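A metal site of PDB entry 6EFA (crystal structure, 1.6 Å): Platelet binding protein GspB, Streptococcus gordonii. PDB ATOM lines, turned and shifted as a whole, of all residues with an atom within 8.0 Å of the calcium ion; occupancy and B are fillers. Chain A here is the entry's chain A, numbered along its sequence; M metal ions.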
ATOM      1  N   ASP A   2     -20.282  -2.593  18.830  1.00  0.00           N
ATOM      2  CA  ASP A   2     -21.703  -2.416  19.227  1.00  0.00           C
ATOM      3  C   ASP A   2     -22.067  -3.453  20.287  1.00  0.00           C
ATOM      4  O   ASP A   2     -22.343  -4.599  19.932  1.00  0.00           O
ATOM      5  CB  ASP A   2     -22.704  -2.384  18.074  1.00  0.00           C
ATOM      6  CG  ASP A   2     -24.098  -1.932  18.509  1.00  0.00           C
ATOM      7  OD1 ASP A   2     -24.239  -1.593  19.665  1.00  0.00           O
ATOM      8  OD2 ASP A   2     -24.984  -1.898  17.687  1.00  0.00           O
ATOM      9  N   THR A   3     -22.033  -3.017  21.534  1.00  0.00           N
ATOM     10  CA  THR A   3     -22.484  -3.866  22.657  1.00  0.00           C
ATOM     11  C   THR A   3     -23.763  -3.259  23.224  1.00  0.00           C
ATOM     12  O   THR A   3     -24.313  -3.869  24.118  1.00  0.00           O
ATOM     13  CB  THR A   3     -21.406  -3.981  23.725  1.00  0.00           C
ATOM     14  OG1 THR A   3     -20.960  -2.667  24.070  1.00  0.00           O
ATOM     15  CG2 THR A   3     -20.232  -4.813  23.257  1.00  0.00           C
ATOM     16  N   GLU A   4     -24.215  -2.109  22.704  1.00  0.00           N
ATOM     17  CA  GLU A   4     -25.422  -1.431  23.235  1.00  0.00           C
ATOM     18  C   GLU A   4     -26.690  -2.075  22.665  1.00  0.00           C
ATOM     19  O   GLU A   4     -26.776  -2.234  21.478  1.00  0.00           O
ATOM     20  CB  GLU A   4     -25.400   0.065  22.928  1.00  0.00           C
ATOM     21  CG  GLU A   4     -26.483   0.835  23.641  1.00  0.00           C
ATOM     22  CD  GLU A   4     -26.502   2.308  23.309  1.00  0.00           C
ATOM     23  OE1 GLU A   4     -27.543   2.838  22.938  1.00  0.00           O
ATOM     24  OE2 GLU A   4     -25.461   2.903  23.414  1.00  0.00           O
ATOM     25  N   ARG A   5     -27.636  -2.375  23.537  1.00  0.00           N
ATOM     26  CA  ARG A   5     -28.809  -3.078  23.071  1.00  0.00           C
ATOM     27  C   ARG A   5     -29.831  -2.102  22.494  1.00  0.00           C
ATOM     28  O   ARG A   5     -29.953  -0.980  22.969  1.00  0.00           O
ATOM     29  CB  ARG A   5     -29.451  -3.809  24.266  1.00  0.00           C
ATOM     30  CG  ARG A   5     -28.599  -4.908  24.980  1.00  0.00           C
ATOM     31  CD  ARG A   5     -29.485  -5.349  26.136  1.00  0.00           C
ATOM     32  NE  ARG A   5     -28.890  -6.398  26.925  1.00  0.00           N
ATOM     33  CZ  ARG A   5     -29.608  -7.170  27.757  1.00  0.00           C
ATOM     34  NH1 ARG A   5     -30.963  -7.071  27.779  1.00  0.00           N
ATOM     35  NH2 ARG A   5     -28.978  -8.077  28.488  1.00  0.00           N
ATOM     36  N   PRO A   6     -30.648  -2.561  21.536  1.00  0.00           N
ATOM     37  CA  PRO A   6     -31.751  -1.749  21.046  1.00  0.00           C
ATOM     38  C   PRO A   6     -32.803  -1.582  22.147  1.00  0.00           C
ATOM     39  O   PRO A   6     -32.842  -2.394  23.090  1.00  0.00           O
ATOM     40  CB  PRO A   6     -32.313  -2.595  19.882  1.00  0.00           C
ATOM     41  CG  PRO A   6     -32.016  -4.061  20.267  1.00  0.00           C
ATOM     42  CD  PRO A   6     -30.614  -3.907  20.943  1.00  0.00           C
ATOM     43  N   VAL A   7     -33.565  -0.519  22.077  1.00  0.00           N
ATOM     44  CA  VAL A   7     -34.595  -0.204  23.103  1.00  0.00           C
ATOM     45  C   VAL A   7     -35.947  -0.197  22.430  1.00  0.00           C
ATOM     46  O   VAL A   7     -36.151   0.500  21.409  1.00  0.00           O
ATOM     47  CB  VAL A   7     -34.314   1.183  23.747  1.00  0.00           C
ATOM     48  CG1 VAL A   7     -35.404   1.522  24.790  1.00  0.00           C
ATOM     49  CG2 VAL A   7     -32.919   1.191  24.356  1.00  0.00           C
ATOM     50  N   THR A  29     -35.416   1.576  18.736  1.00  0.00           N
ATOM     51  CA  THR A  29     -34.272   2.420  18.352  1.00  0.00           C
ATOM     52  C   THR A  29     -32.979   1.709  18.705  1.00  0.00           C
ATOM     53  O   THR A  29     -32.973   0.758  19.513  1.00  0.00           O
ATOM     54  CB  THR A  29     -34.316   3.760  19.042  1.00  0.00           C
ATOM     55  OG1 THR A  29     -34.445   3.525  20.427  1.00  0.00           O
ATOM     56  CG2 THR A  29     -35.563   4.522  18.670  1.00  0.00           C
ATOM     57  N   ASP A  30     -31.874   2.132  18.076  1.00  0.00           N
ATOM     58  CA  ASP A  30     -30.591   1.502  18.386  1.00  0.00           C
ATOM     59  C   ASP A  30     -29.501   2.495  18.057  1.00  0.00           C
ATOM     60  O   ASP A  30     -29.624   3.242  17.077  1.00  0.00           O
ATOM     61  CB  ASP A  30     -30.368   0.209  17.616  1.00  0.00           C
ATOM     62  CG  ASP A  30     -29.180  -0.534  18.100  1.00  0.00           C
ATOM     63  OD1 ASP A  30     -29.239  -1.129  19.173  1.00  0.00           O
ATOM     64  OD2 ASP A  30     -28.102  -0.502  17.452  1.00  0.00           O
ATOM     65  N   ASN A  31     -28.439   2.486  18.854  1.00  0.00           N
ATOM     66  CA  ASN A  31     -27.306   3.373  18.575  1.00  0.00           C
ATOM     67  C   ASN A  31     -26.783   3.206  17.143  1.00  0.00           C
ATOM     68  O   ASN A  31     -26.315   4.164  16.536  1.00  0.00           O
ATOM     69  CB  ASN A  31     -26.157   3.146  19.578  1.00  0.00           C
ATOM     70  CG  ASN A  31     -25.703   1.700  19.648  1.00  0.00           C
ATOM     71  OD1 ASN A  31     -26.529   0.794  19.771  1.00  0.00           O
ATOM     72  ND2 ASN A  31     -24.402   1.475  19.530  1.00  0.00           N
ATOM     73  N   SER A  32     -26.875   2.003  16.590  1.00  0.00           N
ATOM     74  CA  SER A  32     -26.311   1.717  15.269  1.00  0.00           C
ATOM     75  C   SER A  32     -27.224   2.122  14.130  1.00  0.00           C
ATOM     76  O   SER A  32     -26.789   2.201  12.969  1.00  0.00           O
ATOM     77  CB  SER A  32     -26.017   0.229  15.137  1.00  0.00           C
ATOM     78  OG  SER A  32     -27.224  -0.498  15.002  1.00  0.00           O
ATOM     79  N   ASN A  33     -28.502   2.345  14.472  1.00  0.00           N
ATOM     80  CA  ASN A  33     -29.549   2.544  13.465  1.00  0.00           C
ATOM     81  C   ASN A  33     -29.688   1.368  12.485  1.00  0.00           C
ATOM     82  O   ASN A  33     -30.265   1.534  11.425  1.00  0.00           O
ATOM     83  CB  ASN A  33     -29.283   3.818  12.672  1.00  0.00           C
ATOM     84  CG  ASN A  33     -29.165   5.002  13.550  1.00  0.00           C
ATOM     85  OD1 ASN A  33     -29.898   5.116  14.502  1.00  0.00           O
ATOM     86  ND2 ASN A  33     -28.218   5.905  13.248  1.00  0.00           N
ATOM     87  N   ALA A  34     -29.203   0.191  12.828  1.00  0.00           N
ATOM     88  CA  ALA A  34     -29.309  -0.932  11.907  1.00  0.00           C
ATOM     89  C   ALA A  34     -29.923  -2.108  12.622  1.00  0.00           C
ATOM     90  O   ALA A  34     -29.518  -2.429  13.763  1.00  0.00           O
ATOM     91  CB  ALA A  34     -27.956  -1.316  11.320  1.00  0.00           C
ATOM     92  N   PHE A  35     -30.870  -2.765  11.939  1.00  0.00           N
ATOM     93  CA  PHE A  35     -31.670  -3.759  12.619  1.00  0.00           C
ATOM     94  C   PHE A  35     -31.724  -5.007  11.827  1.00  0.00           C
ATOM     95  O   PHE A  35     -31.446  -5.028  10.636  1.00  0.00           O
ATOM     96  CB  PHE A  35     -33.103  -3.239  12.827  1.00  0.00           C
ATOM     97  CG  PHE A  35     -33.174  -1.981  13.585  1.00  0.00           C
ATOM     98  CD1 PHE A  35     -33.130  -0.760  12.942  1.00  0.00           C
ATOM     99  CD2 PHE A  35     -33.295  -2.016  14.982  1.00  0.00           C
ATOM    100  CE1 PHE A  35     -33.221   0.426  13.664  1.00  0.00           C
ATOM    101  CE2 PHE A  35     -33.364  -0.826  15.725  1.00  0.00           C
ATOM    102  CZ  PHE A  35     -33.319   0.376  15.074  1.00  0.00           C
ATOM    103  N   THR A  92     -34.052  -7.162  17.619  1.00  0.00           N
ATOM    104  CA  THR A  92     -32.651  -7.485  17.428  1.00  0.00           C
ATOM    105  C   THR A  92     -31.986  -6.427  16.552  1.00  0.00           C
ATOM    106  O   THR A  92     -32.534  -6.079  15.495  1.00  0.00           O
ATOM    107  CB  THR A  92     -32.472  -8.887  16.740  1.00  0.00           C
ATOM    108  OG1 THR A  92     -33.273  -9.881  17.420  1.00  0.00           O
ATOM    109  CG2 THR A  92     -30.966  -9.298  16.727  1.00  0.00           C
ATOM    110  N   ASP A  93     -30.825  -5.950  16.964  1.00  0.00           N
ATOM    111  CA  ASP A  93     -30.122  -5.001  16.095  1.00  0.00           C
ATOM    112  C   ASP A  93     -29.248  -5.788  15.111  1.00  0.00           C
ATOM    113  O   ASP A  93     -29.228  -7.019  15.127  1.00  0.00           O
ATOM    114  CB  ASP A  93     -29.303  -3.923  16.872  1.00  0.00           C
ATOM    115  CG  ASP A  93     -28.142  -4.486  17.689  1.00  0.00           C
ATOM    116  OD1 ASP A  93     -27.717  -5.630  17.480  1.00  0.00           O
ATOM    117  OD2 ASP A  93     -27.625  -3.737  18.551  1.00  0.00           O
ATOM    118  N   ALA A  94     -28.606  -5.079  14.189  1.00  0.00           N
ATOM    119  CA  ALA A  94     -27.837  -5.757  13.143  1.00  0.00           C
ATOM    120  C   ALA A  94     -26.693  -6.584  13.730  1.00  0.00           C
ATOM    121  O   ALA A  94     -26.387  -7.670  13.202  1.00  0.00           O
ATOM    122  CB  ALA A  94     -27.311  -4.759  12.165  1.00  0.00           C
ATOM    123  N   ALA A  95     -26.097  -6.090  14.806  1.00  0.00           N
ATOM    124  CA  ALA A  95     -24.999  -6.784  15.516  1.00  0.00           C
ATOM    125  C   ALA A  95     -25.453  -8.026  16.271  1.00  0.00           C
ATOM    126  O   ALA A  95     -24.608  -8.819  16.726  1.00  0.00           O
ATOM    127  CB  ALA A  95     -24.264  -5.831  16.471  1.00  0.00           C
ATOM    128  N   GLY A  96     -26.775  -8.195  16.433  1.00  0.00           N
ATOM    129  CA  GLY A  96     -27.312  -9.349  17.124  1.00  0.00           C
ATOM    130  C   GLY A  96     -27.687  -9.095  18.591  1.00  0.00           C
ATOM    131  O   GLY A  96     -28.066 -10.049  19.275  1.00  0.00           O
ATOM    132  N   ASN A  97     -27.491  -7.886  19.080  1.00  0.00           N
ATOM    133  CA  ASN A  97     -27.895  -7.532  20.428  1.00  0.00           C
ATOM    134  C   ASN A  97     -29.432  -7.505  20.489  1.00  0.00           C
ATOM    135  O   ASN A  97     -30.105  -7.090  19.528  1.00  0.00           O
ATOM    136  CB  ASN A  97     -27.365  -6.174  20.833  1.00  0.00           C
ATOM    137  CG  ASN A  97     -25.834  -6.068  20.705  1.00  0.00           C
ATOM    138  OD1 ASN A  97     -25.099  -6.724  21.434  1.00  0.00           O
ATOM    139  ND2 ASN A  97     -25.396  -5.163  19.876  1.00  0.00           N
ATOM    140  N   VAL A  98     -29.989  -7.985  21.597  1.00  0.00           N
ATOM    141  CA  VAL A  98     -31.466  -7.989  21.822  1.00  0.00           C
ATOM    142  C   VAL A  98     -31.780  -7.117  23.003  1.00  0.00           C
ATOM    143  O   VAL A  98     -30.948  -6.968  23.903  1.00  0.00           O
ATOM    144  CB  VAL A  98     -31.977  -9.371  22.054  1.00  0.00           C
ATOM    145  CG1 VAL A  98     -31.768 -10.193  20.766  1.00  0.00           C
ATOM    146  CG2 VAL A  98     -31.301 -10.025  23.267  1.00  0.00           C
HETATM  147 CA    CA M   1     -26.819  -1.521  19.329  1.00  0.00          CA
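The side-chain hydroxyl (OG) of Ser 32 sits close to the side-chain carboxylate (OD2) of Asp 30, 2.6 Å away.
The backbone carbonyl oxygen (O) of Asp 30 lies close to the side-chain amide oxygen (OD1) of Asn 33 (3.2 Å).
The side-chain carboxylate of Asp 93 sits at hydrogen-bond distance from the backbone NH of Asn 97 (2.8 Å).
The backbone NH of Ala 95 lies within hydrogen-bond range of the side-chain carboxylate of Asp 93, at 3.2 Å.
The side-chain carboxylate (OD1) of Asp 93 is in hydrogen-bond range of the backbone NH (N) of Gly 96 (2.9 Å).
ND2 of Asn 97 is in hydrogen-bond range of O of Asp 2 (3.1 Å).
Residues that only touch the calcium ion: Asn 97.
Within 4 Å of the calcium ion: Asp 2, Glu 4, Asp 30, Asn 31, Asp 93 and Asn 97.
The calcium ion is bound by O of Glu 4 (2.3 Å), OD1 of Asn 31 (2.4 Å), OD1 of Asp 30 (2.5 Å), OD2 of Asp 93 (2.5 Å), OD2 of Asp 2 (2.5 Å), OD2 of Asp 30 (2.5 Å) and OD1 of Asp 2 (2.6 Å).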
